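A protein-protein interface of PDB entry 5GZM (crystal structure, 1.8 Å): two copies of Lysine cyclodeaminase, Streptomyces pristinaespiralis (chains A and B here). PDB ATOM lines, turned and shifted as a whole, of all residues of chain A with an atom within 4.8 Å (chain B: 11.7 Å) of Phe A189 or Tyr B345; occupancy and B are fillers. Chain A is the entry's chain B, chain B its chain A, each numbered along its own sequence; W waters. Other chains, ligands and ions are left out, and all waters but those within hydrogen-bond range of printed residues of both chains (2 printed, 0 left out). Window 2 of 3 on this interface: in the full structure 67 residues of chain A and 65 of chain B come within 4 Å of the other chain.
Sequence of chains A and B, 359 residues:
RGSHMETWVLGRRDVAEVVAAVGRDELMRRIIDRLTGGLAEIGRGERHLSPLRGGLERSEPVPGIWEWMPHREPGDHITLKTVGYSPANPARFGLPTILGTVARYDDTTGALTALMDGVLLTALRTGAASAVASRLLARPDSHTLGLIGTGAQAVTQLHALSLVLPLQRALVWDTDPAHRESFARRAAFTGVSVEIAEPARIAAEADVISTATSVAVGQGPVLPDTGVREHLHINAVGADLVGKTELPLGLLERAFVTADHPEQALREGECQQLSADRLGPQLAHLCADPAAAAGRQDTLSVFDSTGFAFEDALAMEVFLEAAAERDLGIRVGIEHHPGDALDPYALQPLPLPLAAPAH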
ATOM      1  N   VAL A  19     -32.138  11.137 -31.161  1.00  0.00           N
ATOM      2  CA  VAL A  19     -31.308  10.998 -29.985  1.00  0.00           C
ATOM      3  C   VAL A  19     -31.992  10.002 -29.058  1.00  0.00           C
ATOM      4  O   VAL A  19     -31.304   9.177 -28.420  1.00  0.00           O
ATOM      5  CB  VAL A  19     -31.135  12.364 -29.235  1.00  0.00           C
ATOM      6  CG1 VAL A  19     -30.436  12.167 -27.888  1.00  0.00           C
ATOM      7  CG2 VAL A  19     -30.390  13.350 -30.079  1.00  0.00           C
ATOM      8  N   ARG A  24     -28.217   8.948 -26.136  1.00  0.00           N
ATOM      9  CA  ARG A  24     -27.190   9.988 -26.193  1.00  0.00           C
ATOM     10  C   ARG A  24     -25.782   9.410 -26.287  1.00  0.00           C
ATOM     11  O   ARG A  24     -24.949   9.885 -27.092  1.00  0.00           O
ATOM     12  CB  ARG A  24     -27.282  10.875 -24.955  1.00  0.00           C
ATOM     13  CG  ARG A  24     -28.513  11.750 -24.931  1.00  0.00           C
ATOM     14  CD  ARG A  24     -28.374  12.689 -23.783  1.00  0.00           C
ATOM     15  NE  ARG A  24     -29.588  13.409 -23.549  1.00  0.00           N
ATOM     16  CZ  ARG A  24     -29.742  14.322 -22.607  1.00  0.00           C
ATOM     17  NH1 ARG A  24     -28.730  14.632 -21.826  1.00  0.00           N
ATOM     18  NH2 ARG A  24     -30.909  14.935 -22.453  1.00  0.00           N
ATOM     19  N   MET A  28     -23.293   9.680 -29.771  1.00  0.00           N
ATOM     20  CA  MET A  28     -21.961  10.243 -29.621  1.00  0.00           C
ATOM     21  C   MET A  28     -20.863   9.289 -30.029  1.00  0.00           C
ATOM     22  O   MET A  28     -19.935   9.653 -30.808  1.00  0.00           O
ATOM     23  CB  MET A  28     -21.714  10.804 -28.192  1.00  0.00           C
ATOM     24  CG  MET A  28     -20.381  11.559 -28.064  1.00  0.00           C
ATOM     25  SD  MET A  28     -20.147  13.044 -29.122  1.00  0.00           S
ATOM     26  CE  MET A  28     -20.964  14.259 -28.089  1.00  0.00           C
ATOM     27  N   LEU A 120     -27.687  20.781 -33.061  1.00  0.00           N
ATOM     28  CA  LEU A 120     -27.266  19.581 -32.316  1.00  0.00           C
ATOM     29  C   LEU A 120     -26.075  18.954 -32.965  1.00  0.00           C
ATOM     30  O   LEU A 120     -25.061  18.593 -32.323  1.00  0.00           O
ATOM     31  CB  LEU A 120     -28.409  18.597 -32.181  1.00  0.00           C
ATOM     32  CG  LEU A 120     -28.079  17.297 -31.415  1.00  0.00           C
ATOM     33  CD1 LEU A 120     -27.739  17.569 -29.965  1.00  0.00           C
ATOM     34  CD2 LEU A 120     -29.235  16.314 -31.493  1.00  0.00           C
ATOM     35  N   LEU A 124     -22.495  17.966 -31.326  1.00  0.00           N
ATOM     36  CA  LEU A 124     -22.029  16.586 -31.242  1.00  0.00           C
ATOM     37  C   LEU A 124     -20.690  16.335 -31.944  1.00  0.00           C
ATOM     38  O   LEU A 124     -19.805  15.719 -31.369  1.00  0.00           O
ATOM     39  CB  LEU A 124     -23.067  15.649 -31.837  1.00  0.00           C
ATOM     40  CG  LEU A 124     -24.397  15.606 -31.098  1.00  0.00           C
ATOM     41  CD1 LEU A 124     -25.360  14.646 -31.764  1.00  0.00           C
ATOM     42  CD2 LEU A 124     -24.175  15.200 -29.667  1.00  0.00           C
ATOM     43  N   VAL A 155     -21.052  21.445 -22.856  1.00  0.00           N
ATOM     44  CA  VAL A 155     -21.865  20.309 -22.546  1.00  0.00           C
ATOM     45  C   VAL A 155     -21.412  19.086 -23.319  1.00  0.00           C
ATOM     46  O   VAL A 155     -21.283  17.998 -22.746  1.00  0.00           O
ATOM     47  CB  VAL A 155     -23.358  20.591 -22.827  1.00  0.00           C
ATOM     48  CG1 VAL A 155     -24.167  19.320 -22.654  1.00  0.00           C
ATOM     49  CG2 VAL A 155     -23.874  21.709 -21.904  1.00  0.00           C
ATOM     50  N   THR A 156     -21.244  19.236 -24.634  1.00  0.00           N
ATOM     51  CA  THR A 156     -20.867  18.050 -25.427  1.00  0.00           C
ATOM     52  C   THR A 156     -19.362  17.778 -25.346  1.00  0.00           C
ATOM     53  O   THR A 156     -18.949  16.638 -25.588  1.00  0.00           O
ATOM     54  CB  THR A 156     -21.266  18.168 -26.901  1.00  0.00           C
ATOM     55  OG1 THR A 156     -20.733  19.365 -27.431  1.00  0.00           O
ATOM     56  CG2 THR A 156     -22.725  18.189 -27.021  1.00  0.00           C
ATOM     57  N   HIS A 159     -19.498  15.601 -22.327  1.00  0.00           N
ATOM     58  CA  HIS A 159     -20.107  14.361 -22.689  1.00  0.00           C
ATOM     59  C   HIS A 159     -19.166  13.462 -23.484  1.00  0.00           C
ATOM     60  O   HIS A 159     -18.901  12.308 -23.075  1.00  0.00           O
ATOM     61  CB  HIS A 159     -21.446  14.566 -23.408  1.00  0.00           C
ATOM     62  CG  HIS A 159     -22.166  13.280 -23.712  1.00  0.00           C
ATOM     63  ND1 HIS A 159     -22.898  13.090 -24.869  1.00  0.00           N
ATOM     64  CD2 HIS A 159     -22.258  12.126 -23.011  1.00  0.00           C
ATOM     65  CE1 HIS A 159     -23.410  11.869 -24.871  1.00  0.00           C
ATOM     66  NE2 HIS A 159     -23.034  11.262 -23.751  1.00  0.00           N
ATOM     67  N   ARG A 186     -26.772  20.901 -16.485  1.00  0.00           N
ATOM     68  CA  ARG A 186     -26.640  20.495 -17.882  1.00  0.00           C
ATOM     69  C   ARG A 186     -25.698  19.322 -18.056  1.00  0.00           C
ATOM     70  O   ARG A 186     -25.797  18.567 -19.039  1.00  0.00           O
ATOM     71  CB  ARG A 186     -26.248  21.710 -18.774  1.00  0.00           C
ATOM     72  CG  ARG A 186     -27.350  22.769 -18.850  1.00  0.00           C
ATOM     73  CD  ARG A 186     -26.982  23.971 -19.713  1.00  0.00           C
ATOM     74  NE  ARG A 186     -26.160  24.906 -18.988  1.00  0.00           N
ATOM     75  CZ  ARG A 186     -24.915  25.290 -19.283  1.00  0.00           C
ATOM     76  NH1 ARG A 186     -24.300  24.943 -20.412  1.00  0.00           N
ATOM     77  NH2 ARG A 186     -24.315  26.130 -18.470  1.00  0.00           N
ATOM     78  N   ALA A 187     -24.837  19.101 -17.083  1.00  0.00           N
ATOM     79  CA  ALA A 187     -23.829  18.065 -17.141  1.00  0.00           C
ATOM     80  C   ALA A 187     -24.262  16.802 -16.335  1.00  0.00           C
ATOM     81  O   ALA A 187     -23.654  15.757 -16.492  1.00  0.00           O
ATOM     82  CB  ALA A 187     -22.550  18.604 -16.552  1.00  0.00           C
ATOM     83  N   ALA A 188     -25.299  16.917 -15.502  1.00  0.00           N
ATOM     84  CA  ALA A 188     -25.619  15.860 -14.505  1.00  0.00           C
ATOM     85  C   ALA A 188     -25.876  14.479 -15.133  1.00  0.00           C
ATOM     86  O   ALA A 188     -25.566  13.469 -14.519  1.00  0.00           O
ATOM     87  CB  ALA A 188     -26.815  16.277 -13.638  1.00  0.00           C
ATOM     88  N   PHE A 189     -26.411  14.436 -16.348  1.00  0.00           N
ATOM     89  CA  PHE A 189     -26.675  13.187 -17.034  1.00  0.00           C
ATOM     90  C   PHE A 189     -25.433  12.339 -17.234  1.00  0.00           C
ATOM     91  O   PHE A 189     -25.546  11.111 -17.391  1.00  0.00           O
ATOM     92  CB  PHE A 189     -27.387  13.404 -18.342  1.00  0.00           C
ATOM     93  CG  PHE A 189     -26.505  13.841 -19.453  1.00  0.00           C
ATOM     94  CD1 PHE A 189     -26.138  15.161 -19.582  1.00  0.00           C
ATOM     95  CD2 PHE A 189     -26.039  12.927 -20.381  1.00  0.00           C
ATOM     96  CE1 PHE A 189     -25.359  15.591 -20.640  1.00  0.00           C
ATOM     97  CE2 PHE A 189     -25.227  13.369 -21.424  1.00  0.00           C
ATOM     98  CZ  PHE A 189     -24.917  14.686 -21.557  1.00  0.00           C
ATOM     99  N   THR A 190     -24.259  12.975 -17.226  1.00  0.00           N
ATOM    100  CA  THR A 190     -23.018  12.260 -17.557  1.00  0.00           C
ATOM    101  C   THR A 190     -22.490  11.506 -16.364  1.00  0.00           C
ATOM    102  O   THR A 190     -21.602  10.662 -16.515  1.00  0.00           O
ATOM    103  CB  THR A 190     -21.861  13.198 -18.011  1.00  0.00           C
ATOM    104  OG1 THR A 190     -21.408  14.001 -16.932  1.00  0.00           O
ATOM    105  CG2 THR A 190     -22.301  14.163 -19.173  1.00  0.00           C
ATOM    106  N   GLY A 191     -22.998  11.846 -15.169  1.00  0.00           N
ATOM    107  CA  GLY A 191     -22.455  11.338 -13.902  1.00  0.00           C
ATOM    108  C   GLY A 191     -21.116  11.927 -13.419  1.00  0.00           C
ATOM    109  O   GLY A 191     -20.549  11.450 -12.462  1.00  0.00           O
ATOM    110  N   HIS B 336     -32.862  23.391 -34.380  1.00  0.00           N
ATOM    111  CA  HIS B 336     -33.090  23.099 -33.001  1.00  0.00           C
ATOM    112  C   HIS B 336     -32.808  24.366 -32.200  1.00  0.00           C
ATOM    113  O   HIS B 336     -31.700  24.938 -32.278  1.00  0.00           O
ATOM    114  CB  HIS B 336     -32.198  21.923 -32.617  1.00  0.00           C
ATOM    115  CG  HIS B 336     -32.085  21.624 -31.151  1.00  0.00           C
ATOM    116  ND1 HIS B 336     -33.160  21.560 -30.291  1.00  0.00           N
ATOM    117  CD2 HIS B 336     -30.995  21.296 -30.415  1.00  0.00           C
ATOM    118  CE1 HIS B 336     -32.732  21.227 -29.082  1.00  0.00           C
ATOM    119  NE2 HIS B 336     -31.420  21.064 -29.134  1.00  0.00           N
ATOM    120  N   HIS B 337     -33.843  24.835 -31.511  1.00  0.00           N
ATOM    121  CA  HIS B 337     -33.745  25.964 -30.582  1.00  0.00           C
ATOM    122  C   HIS B 337     -34.046  25.467 -29.173  1.00  0.00           C
ATOM    123  O   HIS B 337     -35.180  25.593 -28.711  1.00  0.00           O
ATOM    124  CB  HIS B 337     -34.709  27.081 -30.939  1.00  0.00           C
ATOM    125  CG  HIS B 337     -34.454  27.695 -32.274  1.00  0.00           C
ATOM    126  ND1 HIS B 337     -35.374  28.499 -32.911  1.00  0.00           N
ATOM    127  CD2 HIS B 337     -33.401  27.592 -33.115  1.00  0.00           C
ATOM    128  CE1 HIS B 337     -34.899  28.873 -34.084  1.00  0.00           C
ATOM    129  NE2 HIS B 337     -33.712  28.315 -34.243  1.00  0.00           N
ATOM    130  N   PRO B 338     -33.026  24.967 -28.461  1.00  0.00           N
ATOM    131  CA  PRO B 338     -33.342  24.343 -27.172  1.00  0.00           C
ATOM    132  C   PRO B 338     -33.913  25.325 -26.163  1.00  0.00           C
ATOM    133  O   PRO B 338     -33.552  26.512 -26.158  1.00  0.00           O
ATOM    134  CB  PRO B 338     -32.006  23.750 -26.728  1.00  0.00           C
ATOM    135  CG  PRO B 338     -30.993  24.535 -27.444  1.00  0.00           C
ATOM    136  CD  PRO B 338     -31.601  24.821 -28.782  1.00  0.00           C
ATOM    137  N   GLY B 339     -34.811  24.849 -25.296  1.00  0.00           N
ATOM    138  CA  GLY B 339     -35.467  25.744 -24.332  1.00  0.00           C
ATOM    139  C   GLY B 339     -34.427  26.400 -23.440  1.00  0.00           C
ATOM    140  O   GLY B 339     -34.603  27.495 -22.965  1.00  0.00           O
ATOM    141  N   ASP B 340     -33.295  25.743 -23.261  1.00  0.00           N
ATOM    142  CA  ASP B 340     -32.182  26.365 -22.576  1.00  0.00           C
ATOM    143  C   ASP B 340     -31.115  26.530 -23.655  1.00  0.00           C
ATOM    144  O   ASP B 340     -30.623  25.530 -24.196  1.00  0.00           O
ATOM    145  CB  ASP B 340     -31.704  25.389 -21.474  1.00  0.00           C
ATOM    146  CG  ASP B 340     -30.406  25.775 -20.824  1.00  0.00           C
ATOM    147  OD1 ASP B 340     -29.737  26.706 -21.282  1.00  0.00           O
ATOM    148  OD2 ASP B 340     -30.039  25.076 -19.824  1.00  0.00           O
ATOM    149  N   ALA B 341     -30.781  27.769 -23.979  1.00  0.00           N
ATOM    150  CA  ALA B 341     -29.890  28.074 -25.141  1.00  0.00           C
ATOM    151  C   ALA B 341     -28.475  27.512 -24.987  1.00  0.00           C
ATOM    152  O   ALA B 341     -27.713  27.366 -25.950  1.00  0.00           O
ATOM    153  CB  ALA B 341     -29.808  29.595 -25.332  1.00  0.00           C
ATOM    154  N   LEU B 342     -28.131  27.194 -23.754  1.00  0.00           N
ATOM    155  CA  LEU B 342     -26.850  26.612 -23.426  1.00  0.00           C
ATOM    156  C   LEU B 342     -26.827  25.101 -23.309  1.00  0.00           C
ATOM    157  O   LEU B 342     -25.817  24.531 -22.884  1.00  0.00           O
ATOM    158  CB  LEU B 342     -26.368  27.256 -22.111  1.00  0.00           C
ATOM    159  CG  LEU B 342     -26.292  28.775 -22.051  1.00  0.00           C
ATOM    160  CD1 LEU B 342     -25.629  29.153 -20.723  1.00  0.00           C
ATOM    161  CD2 LEU B 342     -25.538  29.438 -23.218  1.00  0.00           C
ATOM    162  N   ASP B 343     -27.902  24.426 -23.699  1.00  0.00           N
ATOM    163  CA  ASP B 343     -28.021  22.994 -23.575  1.00  0.00           C
ATOM    164  C   ASP B 343     -28.463  22.337 -24.880  1.00  0.00           C
ATOM    165  O   ASP B 343     -29.680  22.234 -25.160  1.00  0.00           O
ATOM    166  CB  ASP B 343     -29.050  22.643 -22.494  1.00  0.00           C
ATOM    167  CG  ASP B 343     -29.101  21.169 -22.189  1.00  0.00           C
ATOM    168  OD1 ASP B 343     -28.334  20.375 -22.776  1.00  0.00           O
ATOM    169  OD2 ASP B 343     -29.854  20.792 -21.262  1.00  0.00           O
ATOM    170  N   PRO B 344     -27.505  21.878 -25.663  1.00  0.00           N
ATOM    171  CA  PRO B 344     -27.797  21.205 -26.923  1.00  0.00           C
ATOM    172  C   PRO B 344     -28.723  20.037 -26.728  1.00  0.00           C
ATOM    173  O   PRO B 344     -29.441  19.666 -27.669  1.00  0.00           O
ATOM    174  CB  PRO B 344     -26.423  20.711 -27.402  1.00  0.00           C
ATOM    175  CG  PRO B 344     -25.432  21.575 -26.709  1.00  0.00           C
ATOM    176  CD  PRO B 344     -26.039  21.950 -25.402  1.00  0.00           C
ATOM    177  N   TYR B 345     -28.703  19.415 -25.543  1.00  0.00           N
ATOM    178  CA  TYR B 345     -29.576  18.226 -25.328  1.00  0.00           C
ATOM    179  C   TYR B 345     -30.982  18.537 -24.778  1.00  0.00           C
ATOM    180  O   TYR B 345     -31.775  17.632 -24.556  1.00  0.00           O
ATOM    181  CB  TYR B 345     -28.885  17.213 -24.434  1.00  0.00           C
ATOM    182  CG  TYR B 345     -27.718  16.519 -25.055  1.00  0.00           C
ATOM    183  CD1 TYR B 345     -27.872  15.755 -26.213  1.00  0.00           C
ATOM    184  CD2 TYR B 345     -26.456  16.578 -24.455  1.00  0.00           C
ATOM    185  CE1 TYR B 345     -26.789  15.068 -26.769  1.00  0.00           C
ATOM    186  CE2 TYR B 345     -25.356  15.924 -24.978  1.00  0.00           C
ATOM    187  CZ  TYR B 345     -25.530  15.133 -26.123  1.00  0.00           C
ATOM    188  OH  TYR B 345     -24.455  14.482 -26.656  1.00  0.00           O
ATOM    189  N   ALA B 346     -31.323  19.801 -24.598  1.00  0.00           N
ATOM    190  CA  ALA B 346     -32.704  20.166 -24.215  1.00  0.00           C
ATOM    191  C   ALA B 346     -33.643  20.056 -25.440  1.00  0.00           C
ATOM    192  O   ALA B 346     -33.988  21.043 -26.122  1.00  0.00           O
ATOM    193  CB  ALA B 346     -32.719  21.544 -23.587  1.00  0.00           C
ATOM    194  N   LEU B 347     -33.992  18.812 -25.744  1.00  0.00           N
ATOM    195  CA  LEU B 347     -34.596  18.445 -26.994  1.00  0.00           C
ATOM    196  C   LEU B 347     -36.090  18.217 -26.705  1.00  0.00           C
ATOM    197  O   LEU B 347     -36.436  17.675 -25.685  1.00  0.00           O
ATOM    198  CB  LEU B 347     -33.968  17.161 -27.558  1.00  0.00           C
ATOM    199  CG  LEU B 347     -32.582  17.501 -28.143  1.00  0.00           C
ATOM    200  CD1 LEU B 347     -31.660  16.335 -27.917  1.00  0.00           C
ATOM    201  CD2 LEU B 347     -32.746  17.842 -29.591  1.00  0.00           C
ATOM    202  N   GLN B 348     -36.979  18.606 -27.595  1.00  0.00           N
ATOM    203  CA  GLN B 348     -38.390  18.277 -27.349  1.00  0.00           C
ATOM    204  C   GLN B 348     -38.939  17.361 -28.429  1.00  0.00           C
ATOM    205  O   GLN B 348     -38.964  17.740 -29.590  1.00  0.00           O
ATOM    206  CB  GLN B 348     -39.202  19.553 -27.310  1.00  0.00           C
ATOM    207  CG  GLN B 348     -40.583  19.376 -26.739  1.00  0.00           C
ATOM    208  CD  GLN B 348     -40.901  20.473 -25.744  1.00  0.00           C
ATOM    209  OE1 GLN B 348     -40.973  21.658 -26.104  1.00  0.00           O
ATOM    210  NE2 GLN B 348     -41.062  20.095 -24.480  1.00  0.00           N
ATOM    211  N   PRO B 349     -39.399  16.173 -28.052  1.00  0.00           N
ATOM    212  CA  PRO B 349     -39.890  15.211 -29.026  1.00  0.00           C
ATOM    213  C   PRO B 349     -41.267  15.580 -29.563  1.00  0.00           C
ATOM    214  O   PRO B 349     -41.867  16.586 -29.152  1.00  0.00           O
ATOM    215  CB  PRO B 349     -39.941  13.911 -28.220  1.00  0.00           C
ATOM    216  CG  PRO B 349     -40.232  14.368 -26.863  1.00  0.00           C
ATOM    217  CD  PRO B 349     -39.436  15.625 -26.688  1.00  0.00           C
HETATM  218  O   HOH W   1     -27.423  18.434 -21.216  1.00  0.00           O
HETATM  219  O   HOH W   2     -25.414  12.316 -28.522  1.00  0.00           O
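No position is printed for both chains. Of the 12 pairs that touch across the chains among the printed residues, none has its exchanged pair printed and touching as well.
Among the printed residues, merely in contact across the chains: Leu A124 with Tyr B345 (3.1 Å), Arg A24 with Tyr B345 (3.5 Å), Leu A120 with Pro B344 (3.5 Å), Val A155 with Leu B342 (3.6 Å), Phe A189 with Tyr B345 (3.7 Å), Arg A186 with Asp B343 (3.7 Å), Met A28 with Tyr B345 (3.8 Å), Val A19 with Leu B347 (3.9 Å) and Val A155 with Pro B344 (3.96 Å).
Of the printed residues of chain B, Leu A120 touches Pro B344. No residue of chain B comes within 4 Å of Thr A156. Of the printed residues of chain B, Arg A186 touches Asp B340, Leu B342 and Asp B343. No residue of chain B comes within 4 Å of Ala A187. Phe A189 touches just one residue of chain B: Tyr B345. No residue of chain B comes within 4 Å of Thr A190. No residue of chain B comes within 4 Å of Gly A191. Gly B339 touches none of the printed residues of chain A. Of the printed residues of chain A, Tyr B345 touches Arg A24, Met A28, Leu A124, His A159 and Phe A189. Pro B349 touches none of the printed residues of chain A. The nearest residue of chain B that does not touch Phe A189 is Asp B343 (6.0 Å).
Water W1 lies within hydrogen-bond range of OD1 of Asp B343 (2.7 Å) and O of Arg A186 (2.7 Å). Water W2 bridges the backbone carbonyl oxygen of Arg A24 (2.9 Å) and the side-chain hydroxyl of Tyr B345 (3.0 Å).
OD1 of Asp B343 sits at hydrogen-bond distance from N of Tyr B345 (3.0 Å). N of Leu B342 lies within hydrogen-bond range of OD1 of Asp B340 (3.0 Å). O of Pro B344 sits at hydrogen-bond distance from NE2 of His B336 (2.8 Å).
Of the 14 printed residues of chain A, 9 touch a printed residue of chain B. Hydrophobic or aromatic side chains of chain A that line the printed part of chain B: Val A19, Met A28, Leu A120, Leu A124, Val A155, His A159 and Phe A189. Among the printed residues, Asp or Glu carboxylates within 4 Å of a Lys or Arg side-chain nitrogen of the other chain: Arg A186 with Asp B340 (3.97 Å).
ND1 of His A159 is in hydrogen-bond range of OH of Tyr B345 (2.7 Å). The side-chain carboxylate (OD2) of Asp B340 lies within salt-bridge range of the guanidinium group (NE) of Arg A186 (3.97 Å). O of Leu B342 lies within hydrogen-bond range of NH1 of Arg A186.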
